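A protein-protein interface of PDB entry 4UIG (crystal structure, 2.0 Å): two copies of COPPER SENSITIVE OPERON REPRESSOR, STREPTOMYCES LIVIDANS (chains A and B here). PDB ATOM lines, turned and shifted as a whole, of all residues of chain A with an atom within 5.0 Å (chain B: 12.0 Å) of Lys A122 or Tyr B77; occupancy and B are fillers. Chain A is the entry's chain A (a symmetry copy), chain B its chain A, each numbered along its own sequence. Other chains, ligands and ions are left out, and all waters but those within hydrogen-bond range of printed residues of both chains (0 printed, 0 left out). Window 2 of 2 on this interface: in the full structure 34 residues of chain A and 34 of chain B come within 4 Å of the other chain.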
ATOM      1  N   HIS A 103     -16.517  17.315 -23.075  1.00  0.00           N
ATOM      2  CA  HIS A 103     -16.863  16.850 -21.729  1.00  0.00           C
ATOM      3  C   HIS A 103     -17.093  17.981 -20.712  1.00  0.00           C
ATOM      4  O   HIS A 103     -18.103  17.979 -19.965  1.00  0.00           O
ATOM      5  CB  HIS A 103     -15.782  15.930 -21.179  1.00  0.00           C
ATOM      6  CG  HIS A 103     -16.124  15.316 -19.857  1.00  0.00           C
ATOM      7  ND1 HIS A 103     -17.141  14.392 -19.708  1.00  0.00           N
ATOM      8  CD2 HIS A 103     -15.616  15.522 -18.621  1.00  0.00           C
ATOM      9  CE1 HIS A 103     -17.216  14.032 -18.434  1.00  0.00           C
ATOM     10  NE2 HIS A 103     -16.301  14.698 -17.759  1.00  0.00           N
ATOM     11  N   CYS A 107     -21.003  17.774 -19.841  1.00  0.00           N
ATOM     12  CA  CYS A 107     -21.118  16.979 -18.628  1.00  0.00           C
ATOM     13  C   CYS A 107     -20.859  17.804 -17.361  1.00  0.00           C
ATOM     14  O   CYS A 107     -21.727  17.889 -16.471  1.00  0.00           O
ATOM     15  CB  CYS A 107     -20.196  15.746 -18.689  1.00  0.00           C
ATOM     16  SG  CYS A 107     -20.777  14.364 -17.674  1.00  0.00           S
ATOM     17  N   VAL A 108     -19.688  18.416 -17.287  1.00  0.00           N
ATOM     18  CA  VAL A 108     -19.292  19.131 -16.086  1.00  0.00           C
ATOM     19  C   VAL A 108     -20.183  20.345 -15.815  1.00  0.00           C
ATOM     20  O   VAL A 108     -20.605  20.557 -14.680  1.00  0.00           O
ATOM     21  CB  VAL A 108     -17.783  19.463 -16.136  1.00  0.00           C
ATOM     22  CG1 VAL A 108     -17.360  20.399 -15.015  1.00  0.00           C
ATOM     23  CG2 VAL A 108     -16.979  18.158 -16.101  1.00  0.00           C
ATOM     24  N   ALA A 111     -23.628  19.278 -14.448  1.00  0.00           N
ATOM     25  CA  ALA A 111     -23.524  18.924 -13.039  1.00  0.00           C
ATOM     26  C   ALA A 111     -23.631  20.115 -12.134  1.00  0.00           C
ATOM     27  O   ALA A 111     -24.194  20.021 -11.025  1.00  0.00           O
ATOM     28  CB  ALA A 111     -22.249  18.177 -12.784  1.00  0.00           C
ATOM     29  N   GLU A 118     -22.684  16.897  -7.033  1.00  0.00           N
ATOM     30  CA  GLU A 118     -22.606  16.437  -8.410  1.00  0.00           C
ATOM     31  C   GLU A 118     -21.406  17.086  -9.112  1.00  0.00           C
ATOM     32  O   GLU A 118     -20.624  16.398  -9.715  1.00  0.00           O
ATOM     33  CB  GLU A 118     -23.870  16.735  -9.171  1.00  0.00           C
ATOM     34  CG  GLU A 118     -25.130  15.948  -8.718  1.00  0.00           C
ATOM     35  CD  GLU A 118     -25.923  16.653  -7.621  1.00  0.00           C
ATOM     36  OE1 GLU A 118     -25.331  17.446  -6.815  1.00  0.00           O
ATOM     37  OE2 GLU A 118     -27.151  16.390  -7.546  1.00  0.00           O
ATOM     38  N   ILE A 119     -21.260  18.408  -9.006  1.00  0.00           N
ATOM     39  CA  ILE A 119     -20.128  19.044  -9.653  1.00  0.00           C
ATOM     40  C   ILE A 119     -18.784  18.585  -9.064  1.00  0.00           C
ATOM     41  O   ILE A 119     -17.863  18.335  -9.814  1.00  0.00           O
ATOM     42  CB  ILE A 119     -20.239  20.600  -9.721  1.00  0.00           C
ATOM     43  CG1 ILE A 119     -19.033  21.187 -10.483  1.00  0.00           C
ATOM     44  CG2 ILE A 119     -20.315  21.230  -8.369  1.00  0.00           C
ATOM     45  CD1 ILE A 119     -19.004  20.785 -11.938  1.00  0.00           C
ATOM     46  N   ASP A 120     -18.677  18.447  -7.754  1.00  0.00           N
ATOM     47  CA  ASP A 120     -17.448  17.944  -7.128  1.00  0.00           C
ATOM     48  C   ASP A 120     -17.062  16.597  -7.662  1.00  0.00           C
ATOM     49  O   ASP A 120     -15.881  16.353  -7.907  1.00  0.00           O
ATOM     50  CB  ASP A 120     -17.573  17.826  -5.619  1.00  0.00           C
ATOM     51  CG  ASP A 120     -17.608  19.189  -4.902  1.00  0.00           C
ATOM     52  OD1 ASP A 120     -17.391  20.238  -5.501  1.00  0.00           O
ATOM     53  OD2 ASP A 120     -17.926  19.211  -3.712  1.00  0.00           O
ATOM     54  N   ALA A 121     -18.049  15.713  -7.844  1.00  0.00           N
ATOM     55  CA  ALA A 121     -17.761  14.351  -8.344  1.00  0.00           C
ATOM     56  C   ALA A 121     -17.283  14.442  -9.798  1.00  0.00           C
ATOM     57  O   ALA A 121     -16.312  13.797 -10.164  1.00  0.00           O
ATOM     58  CB  ALA A 121     -18.987  13.424  -8.242  1.00  0.00           C
ATOM     59  N   LYS A 122     -17.932  15.255 -10.613  1.00  0.00           N
ATOM     60  CA  LYS A 122     -17.512  15.390 -11.986  1.00  0.00           C
ATOM     61  C   LYS A 122     -16.130  16.017 -12.126  1.00  0.00           C
ATOM     62  O   LYS A 122     -15.342  15.592 -12.975  1.00  0.00           O
ATOM     63  CB  LYS A 122     -18.510  16.178 -12.843  1.00  0.00           C
ATOM     64  CG  LYS A 122     -19.771  15.441 -13.162  1.00  0.00           C
ATOM     65  CD  LYS A 122     -19.603  14.335 -14.194  1.00  0.00           C
ATOM     66  CE  LYS A 122     -20.665  13.295 -13.934  1.00  0.00           C
ATOM     67  NZ  LYS A 122     -20.853  12.338 -15.034  1.00  0.00           N
ATOM     68  N   VAL A 123     -15.853  17.034 -11.321  1.00  0.00           N
ATOM     69  CA  VAL A 123     -14.553  17.729 -11.410  1.00  0.00           C
ATOM     70  C   VAL A 123     -13.441  16.819 -10.903  1.00  0.00           C
ATOM     71  O   VAL A 123     -12.419  16.744 -11.535  1.00  0.00           O
ATOM     72  CB  VAL A 123     -14.602  19.075 -10.661  1.00  0.00           C
ATOM     73  CG1 VAL A 123     -13.216  19.632 -10.426  1.00  0.00           C
ATOM     74  CG2 VAL A 123     -15.494  20.042 -11.437  1.00  0.00           C
ATOM     75  N   GLU A 124     -13.684  16.095  -9.816  1.00  0.00           N
ATOM     76  CA  GLU A 124     -12.732  15.094  -9.346  1.00  0.00           C
ATOM     77  C   GLU A 124     -12.375  14.055 -10.433  1.00  0.00           C
ATOM     78  O   GLU A 124     -11.217  13.769 -10.707  1.00  0.00           O
ATOM     79  CB  GLU A 124     -13.224  14.438  -8.031  1.00  0.00           C
ATOM     80  CG  GLU A 124     -12.279  13.358  -7.528  1.00  0.00           C
ATOM     81  CD  GLU A 124     -12.695  12.710  -6.212  1.00  0.00           C
ATOM     82  OE1 GLU A 124     -13.403  13.340  -5.404  1.00  0.00           O
ATOM     83  OE2 GLU A 124     -12.286  11.554  -5.986  1.00  0.00           O
ATOM     84  N   GLU A 125     -13.375  13.534 -11.103  1.00  0.00           N
ATOM     85  CA  GLU A 125     -13.161  12.610 -12.188  1.00  0.00           C
ATOM     86  C   GLU A 125     -12.385  13.214 -13.382  1.00  0.00           C
ATOM     87  O   GLU A 125     -11.470  12.592 -13.959  1.00  0.00           O
ATOM     88  CB  GLU A 125     -14.546  12.126 -12.617  1.00  0.00           C
ATOM     89  CG  GLU A 125     -14.556  11.157 -13.757  1.00  0.00           C
ATOM     90  CD  GLU A 125     -15.966  10.738 -14.147  1.00  0.00           C
ATOM     91  OE1 GLU A 125     -16.801  11.593 -14.550  1.00  0.00           O
ATOM     92  OE2 GLU A 125     -16.215   9.519 -14.086  1.00  0.00           O
ATOM     93  N   ALA A 126     -12.769  14.411 -13.817  1.00  0.00           N
ATOM     94  CA  ALA A 126     -12.093  15.048 -14.954  1.00  0.00           C
ATOM     95  C   ALA A 126     -10.628  15.334 -14.615  1.00  0.00           C
ATOM     96  O   ALA A 126      -9.725  15.200 -15.465  1.00  0.00           O
ATOM     97  CB  ALA A 126     -12.788  16.362 -15.327  1.00  0.00           C
ATOM     98  N   THR A 127     -10.403  15.746 -13.386  1.00  0.00           N
ATOM     99  CA  THR A 127      -9.059  16.102 -12.946  1.00  0.00           C
ATOM    100  C   THR A 127      -8.133  14.840 -12.901  1.00  0.00           C
ATOM    101  O   THR A 127      -7.012  14.906 -13.371  1.00  0.00           O
ATOM    102  CB  THR A 127      -9.167  16.799 -11.580  1.00  0.00           C
ATOM    103  OG1 THR A 127      -9.746  18.091 -11.818  1.00  0.00           O
ATOM    104  CG2 THR A 127      -7.835  16.961 -10.914  1.00  0.00           C
ATOM    105  N   GLY B  67     -10.212   0.118 -31.184  1.00  0.00           N
ATOM    106  CA  GLY B  67     -11.026   0.231 -29.954  1.00  0.00           C
ATOM    107  C   GLY B  67     -11.581   1.616 -29.718  1.00  0.00           C
ATOM    108  O   GLY B  67     -12.765   1.790 -29.413  1.00  0.00           O
ATOM    109  N   LEU B  68     -10.753   2.650 -29.890  1.00  0.00           N
ATOM    110  CA  LEU B  68     -11.199   4.027 -29.745  1.00  0.00           C
ATOM    111  C   LEU B  68     -12.284   4.392 -30.725  1.00  0.00           C
ATOM    112  O   LEU B  68     -13.226   5.124 -30.383  1.00  0.00           O
ATOM    113  CB  LEU B  68     -10.019   5.023 -29.868  1.00  0.00           C
ATOM    114  CG  LEU B  68      -9.037   5.039 -28.709  1.00  0.00           C
ATOM    115  CD1 LEU B  68      -7.813   5.862 -29.153  1.00  0.00           C
ATOM    116  CD2 LEU B  68      -9.692   5.658 -27.465  1.00  0.00           C
ATOM    117  N   GLN B  69     -12.148   3.920 -31.955  1.00  0.00           N
ATOM    118  CA  GLN B  69     -13.180   4.152 -32.963  1.00  0.00           C
ATOM    119  C   GLN B  69     -14.497   3.516 -32.602  1.00  0.00           C
ATOM    120  O   GLN B  69     -15.521   4.164 -32.750  1.00  0.00           O
ATOM    121  CB  GLN B  69     -12.732   3.655 -34.336  1.00  0.00           C
ATOM    122  CG  GLN B  69     -11.670   4.545 -34.933  1.00  0.00           C
ATOM    123  CD  GLN B  69     -10.964   3.916 -36.118  1.00  0.00           C
ATOM    124  OE1 GLN B  69      -9.803   3.539 -36.046  1.00  0.00           O
ATOM    125  NE2 GLN B  69     -11.659   3.831 -37.206  1.00  0.00           N
ATOM    126  N   ARG B  70     -14.449   2.292 -32.070  1.00  0.00           N
ATOM    127  CA  ARG B  70     -15.673   1.629 -31.586  1.00  0.00           C
ATOM    128  C   ARG B  70     -16.321   2.417 -30.423  1.00  0.00           C
ATOM    129  O   ARG B  70     -17.562   2.592 -30.357  1.00  0.00           O
ATOM    130  CB  ARG B  70     -15.392   0.193 -31.171  1.00  0.00           C
ATOM    131  CG  ARG B  70     -15.151  -0.702 -32.392  1.00  0.00           C
ATOM    132  CD  ARG B  70     -15.161  -2.180 -32.063  1.00  0.00           C
ATOM    133  NE  ARG B  70     -14.224  -2.522 -30.989  1.00  0.00           N
ATOM    134  CZ  ARG B  70     -12.928  -2.861 -31.125  1.00  0.00           C
ATOM    135  NH1 ARG B  70     -12.320  -2.940 -32.312  1.00  0.00           N
ATOM    136  NH2 ARG B  70     -12.245  -3.135 -30.024  1.00  0.00           N
ATOM    137  N   MET B  71     -15.482   2.934 -29.524  1.00  0.00           N
ATOM    138  CA  MET B  71     -15.975   3.703 -28.392  1.00  0.00           C
ATOM    139  C   MET B  71     -16.711   4.953 -28.833  1.00  0.00           C
ATOM    140  O   MET B  71     -17.767   5.305 -28.287  1.00  0.00           O
ATOM    141  CB  MET B  71     -14.850   4.062 -27.418  1.00  0.00           C
ATOM    142  CG  MET B  71     -14.227   2.854 -26.728  1.00  0.00           C
ATOM    143  SD  MET B  71     -12.781   3.208 -25.644  1.00  0.00           S
ATOM    144  CE  MET B  71     -13.476   3.333 -24.006  1.00  0.00           C
ATOM    145  N   VAL B  72     -16.111   5.682 -29.762  1.00  0.00           N
ATOM    146  CA  VAL B  72     -16.728   6.863 -30.317  1.00  0.00           C
ATOM    147  C   VAL B  72     -18.026   6.471 -31.075  1.00  0.00           C
ATOM    148  O   VAL B  72     -19.049   7.136 -30.930  1.00  0.00           O
ATOM    149  CB  VAL B  72     -15.778   7.634 -31.251  1.00  0.00           C
ATOM    150  CG1 VAL B  72     -16.524   8.676 -32.041  1.00  0.00           C
ATOM    151  CG2 VAL B  72     -14.657   8.303 -30.457  1.00  0.00           C
ATOM    152  N   ASP B  73     -17.959   5.400 -31.859  1.00  0.00           N
ATOM    153  CA  ASP B  73     -19.120   4.957 -32.634  1.00  0.00           C
ATOM    154  C   ASP B  73     -20.340   4.625 -31.722  1.00  0.00           C
ATOM    155  O   ASP B  73     -21.432   5.028 -32.023  1.00  0.00           O
ATOM    156  CB  ASP B  73     -18.719   3.809 -33.530  1.00  0.00           C
ATOM    157  CG  ASP B  73     -19.612   3.671 -34.748  1.00  0.00           C
ATOM    158  OD1 ASP B  73     -20.298   4.658 -35.167  1.00  0.00           O
ATOM    159  OD2 ASP B  73     -19.599   2.536 -35.268  1.00  0.00           O
ATOM    160  N   GLU B  74     -20.079   4.039 -30.549  1.00  0.00           N
ATOM    161  CA  GLU B  74     -21.074   3.697 -29.555  1.00  0.00           C
ATOM    162  C   GLU B  74     -21.411   4.795 -28.532  1.00  0.00           C
ATOM    163  O   GLU B  74     -22.193   4.547 -27.614  1.00  0.00           O
ATOM    164  CB  GLU B  74     -20.598   2.474 -28.795  1.00  0.00           C
ATOM    165  CG  GLU B  74     -20.404   1.257 -29.663  1.00  0.00           C
ATOM    166  CD  GLU B  74     -19.671   0.135 -28.941  1.00  0.00           C
ATOM    167  OE1 GLU B  74     -19.423   0.221 -27.722  1.00  0.00           O
ATOM    168  OE2 GLU B  74     -19.290  -0.824 -29.590  1.00  0.00           O
ATOM    169  N   ASP B  75     -20.796   5.975 -28.663  1.00  0.00           N
ATOM    170  CA  ASP B  75     -20.916   7.061 -27.712  1.00  0.00           C
ATOM    171  C   ASP B  75     -20.607   6.634 -26.246  1.00  0.00           C
ATOM    172  O   ASP B  75     -21.338   6.963 -25.328  1.00  0.00           O
ATOM    173  CB  ASP B  75     -22.312   7.691 -27.858  1.00  0.00           C
ATOM    174  CG  ASP B  75     -22.456   9.032 -27.126  1.00  0.00           C
ATOM    175  OD1 ASP B  75     -21.468   9.793 -26.986  1.00  0.00           O
ATOM    176  OD2 ASP B  75     -23.594   9.324 -26.703  1.00  0.00           O
ATOM    177  N   VAL B  76     -19.547   5.862 -26.050  1.00  0.00           N
ATOM    178  CA  VAL B  76     -19.016   5.537 -24.729  1.00  0.00           C
ATOM    179  C   VAL B  76     -18.710   6.851 -23.992  1.00  0.00           C
ATOM    180  O   VAL B  76     -18.368   7.875 -24.606  1.00  0.00           O
ATOM    181  CB  VAL B  76     -17.757   4.660 -24.832  1.00  0.00           C
ATOM    182  CG1 VAL B  76     -17.064   4.483 -23.479  1.00  0.00           C
ATOM    183  CG2 VAL B  76     -18.136   3.296 -25.359  1.00  0.00           C
ATOM    184  N   TYR B  77     -18.885   6.825 -22.685  1.00  0.00           N
ATOM    185  CA  TYR B  77     -18.669   7.987 -21.832  1.00  0.00           C
ATOM    186  C   TYR B  77     -17.249   8.538 -22.100  1.00  0.00           C
ATOM    187  O   TYR B  77     -16.302   7.781 -22.092  1.00  0.00           O
ATOM    188  CB  TYR B  77     -18.757   7.558 -20.382  1.00  0.00           C
ATOM    189  CG  TYR B  77     -18.664   8.684 -19.345  1.00  0.00           C
ATOM    190  CD1 TYR B  77     -19.498   9.804 -19.423  1.00  0.00           C
ATOM    191  CD2 TYR B  77     -17.776   8.583 -18.258  1.00  0.00           C
ATOM    192  CE1 TYR B  77     -19.459  10.796 -18.461  1.00  0.00           C
ATOM    193  CE2 TYR B  77     -17.724   9.570 -17.285  1.00  0.00           C
ATOM    194  CZ  TYR B  77     -18.564  10.674 -17.398  1.00  0.00           C
ATOM    195  OH  TYR B  77     -18.496  11.655 -16.446  1.00  0.00           O
ATOM    196  N   CYS B  78     -17.145   9.839 -22.304  1.00  0.00           N
ATOM    197  CA  CYS B  78     -15.878  10.462 -22.659  1.00  0.00           C
ATOM    198  C   CYS B  78     -14.725  10.217 -21.751  1.00  0.00           C
ATOM    199  O   CYS B  78     -13.620  10.031 -22.251  1.00  0.00           O
ATOM    200  CB  CYS B  78     -16.064  11.947 -22.889  1.00  0.00           C
ATOM    201  SG  CYS B  78     -16.862  12.066 -24.491  1.00  0.00           S
ATOM    202  N   ILE B  79     -14.947  10.169 -20.437  1.00  0.00           N
ATOM    203  CA  ILE B  79     -13.866   9.839 -19.550  1.00  0.00           C
ATOM    204  C   ILE B  79     -13.311   8.471 -19.853  1.00  0.00           C
ATOM    205  O   ILE B  79     -12.100   8.274 -19.750  1.00  0.00           O
ATOM    206  CB  ILE B  79     -14.251   9.944 -18.053  1.00  0.00           C
ATOM    207  CG1 ILE B  79     -14.549  11.416 -17.700  1.00  0.00           C
ATOM    208  CG2 ILE B  79     -13.203   9.315 -17.117  1.00  0.00           C
ATOM    209  CD1 ILE B  79     -13.419  12.380 -17.927  1.00  0.00           C
ATOM    210  N   ASP B  80     -14.173   7.501 -20.174  1.00  0.00           N
ATOM    211  CA  ASP B  80     -13.648   6.185 -20.496  1.00  0.00           C
ATOM    212  C   ASP B  80     -12.847   6.197 -21.796  1.00  0.00           C
ATOM    213  O   ASP B  80     -11.865   5.464 -21.914  1.00  0.00           O
ATOM    214  CB  ASP B  80     -14.763   5.120 -20.525  1.00  0.00           C
ATOM    215  CG  ASP B  80     -15.466   4.992 -19.178  1.00  0.00           C
ATOM    216  OD1 ASP B  80     -14.793   5.089 -18.141  1.00  0.00           O
ATOM    217  OD2 ASP B  80     -16.685   4.839 -19.152  1.00  0.00           O
ATOM    218  N   ILE B  81     -13.270   7.005 -22.748  1.00  0.00           N
ATOM    219  CA  ILE B  81     -12.521   7.161 -23.972  1.00  0.00           C
ATOM    220  C   ILE B  81     -11.108   7.750 -23.635  1.00  0.00           C
ATOM    221  O   ILE B  81     -10.076   7.216 -24.052  1.00  0.00           O
ATOM    222  CB  ILE B  81     -13.302   7.962 -24.994  1.00  0.00           C
ATOM    223  CG1 ILE B  81     -14.640   7.255 -25.377  1.00  0.00           C
ATOM    224  CG2 ILE B  81     -12.509   8.098 -26.293  1.00  0.00           C
ATOM    225  CD1 ILE B  81     -15.453   7.990 -26.452  1.00  0.00           C
ATOM    226  N   LEU B  82     -11.070   8.786 -22.812  1.00  0.00           N
ATOM    227  CA  LEU B  82      -9.789   9.373 -22.359  1.00  0.00           C
ATOM    228  C   LEU B  82      -8.858   8.448 -21.695  1.00  0.00           C
ATOM    229  O   LEU B  82      -7.641   8.531 -21.936  1.00  0.00           O
ATOM    230  CB  LEU B  82     -10.047  10.508 -21.392  1.00  0.00           C
ATOM    231  CG  LEU B  82     -10.535  11.742 -22.094  1.00  0.00           C
ATOM    232  CD1 LEU B  82     -10.935  12.749 -21.017  1.00  0.00           C
ATOM    233  CD2 LEU B  82      -9.403  12.321 -22.927  1.00  0.00           C
ATOM    234  N   THR B  83      -9.384   7.568 -20.854  1.00  0.00           N
ATOM    235  CA  THR B  83      -8.587   6.536 -20.247  1.00  0.00           C
ATOM    236  C   THR B  83      -7.884   5.646 -21.294  1.00  0.00           C
ATOM    237  O   THR B  83      -6.677   5.310 -21.129  1.00  0.00           O
ATOM    238  CB  THR B  83      -9.439   5.670 -19.318  1.00  0.00           C
ATOM    239  OG1 THR B  83      -9.929   6.492 -18.270  1.00  0.00           O
ATOM    240  CG2 THR B  83      -8.632   4.555 -18.725  1.00  0.00           C
ATOM    241  N   GLN B  84      -8.605   5.296 -22.371  1.00  0.00           N
ATOM    242  CA  GLN B  84      -8.002   4.508 -23.421  1.00  0.00           C
ATOM    243  C   GLN B  84      -7.033   5.337 -24.266  1.00  0.00           C
ATOM    244  O   GLN B  84      -6.042   4.811 -24.721  1.00  0.00           O
ATOM    245  CB  GLN B  84      -9.049   3.845 -24.304  1.00  0.00           C
ATOM    246  CG  GLN B  84      -8.419   2.849 -25.277  1.00  0.00           C
ATOM    247  CD  GLN B  84      -7.499   1.878 -24.586  1.00  0.00           C
ATOM    248  OE1 GLN B  84      -7.818   1.384 -23.497  1.00  0.00           O
ATOM    249  NE2 GLN B  84      -6.369   1.561 -25.211  1.00  0.00           N
ATOM    250  N   VAL B  85      -7.325   6.619 -24.485  1.00  0.00           N
ATOM    251  CA  VAL B  85      -6.376   7.484 -25.204  1.00  0.00           C
ATOM    252  C   VAL B  85      -5.013   7.519 -24.443  1.00  0.00           C
ATOM    253  O   VAL B  85      -3.933   7.319 -25.015  1.00  0.00           O
ATOM    254  CB  VAL B  85      -6.893   8.908 -25.442  1.00  0.00           C
ATOM    255  CG1 VAL B  85      -5.801   9.843 -26.041  1.00  0.00           C
ATOM    256  CG2 VAL B  85      -8.067   8.914 -26.356  1.00  0.00           C
ATOM    257  N   SER B  86      -5.093   7.676 -23.138  1.00  0.00           N
ATOM    258  CA  SER B  86      -3.930   7.701 -22.309  1.00  0.00           C
ATOM    259  C   SER B  86      -3.171   6.402 -22.305  1.00  0.00           C
ATOM    260  O   SER B  86      -1.947   6.432 -22.350  1.00  0.00           O
ATOM    261  CB  SER B  86      -4.323   8.129 -20.882  1.00  0.00           C
ATOM    262  OG  SER B  86      -4.971   9.390 -20.934  1.00  0.00           O
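The side-chain hydroxyl (OH) of Tyr B77 lies within hydrogen-bond range of the side-chain carboxylate (OE1) of Glu A125 (2.5 Å). The side-chain hydroxyl (OH) of Tyr B77 sits at hydrogen-bond distance from the side-chain amino group (NZ) of Lys A122 (2.8 Å). The side-chain hydroxyl (OH) of Tyr B77 lies within hydrogen-bond range of the side-chain sulfur (SG) of Cys A107 (3.7 Å).
SG of Cys A107 lies within hydrogen-bond range of NZ of Lys A122 (3.3 Å). The side-chain hydroxyl (OG1) of Thr B83 sits at hydrogen-bond distance from the backbone carbonyl oxygen (O) of Ile B79 (3.2 Å). O of His A103 lies within hydrogen-bond range of N of Val A108, at 3.1 Å.
Tyr B77 touches His A103 (OH to CE1, 3.4 Å). Ile B79 touches His A103. Glu A125 touches Ile B79 (OE1 to CG1, 3.9 Å).
Of chain B, only Tyr B77 (2.8 Å) comes within 4 Å of Lys A122. No residue of chain B comes within 4 Å of Val A108. No residue of chain B comes within 4 Å of Ile A119. No residue of chain B comes within 4 Å of Ala A121. No residue of chain B comes within 4 Å of Val A123. Of the printed residues of chain B, Glu A125 touches Tyr B77 (2.5 Å) and Ile B79 (3.9 Å). No residue of chain B comes within 4 Å of Ala A126. Of the printed residues of chain B, His A103 touches Tyr B77 and Ile B79. Printed residues of chain B within 4 Å of Cys A107: Tyr B77. Asp B80 touches none of the printed residues of chain A. Thr A127 touches none of the printed residues of chain B.
Hydrophobic or aromatic side chains of chain A within 4 Å of the printed part of chain B: His A103. Printed residues of chain B that touch a printed residue of chain A: Tyr B77 and Ile B79. Hydrophobic or aromatic side chains of chain B within 4 Å of the printed part of chain A: Tyr B77 and Ile B79. Among the printed residues, no Asp or Glu carboxylate lies within 4 Å of a Lys or Arg side-chain nitrogen of the other chain.
No position is printed for both chains.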
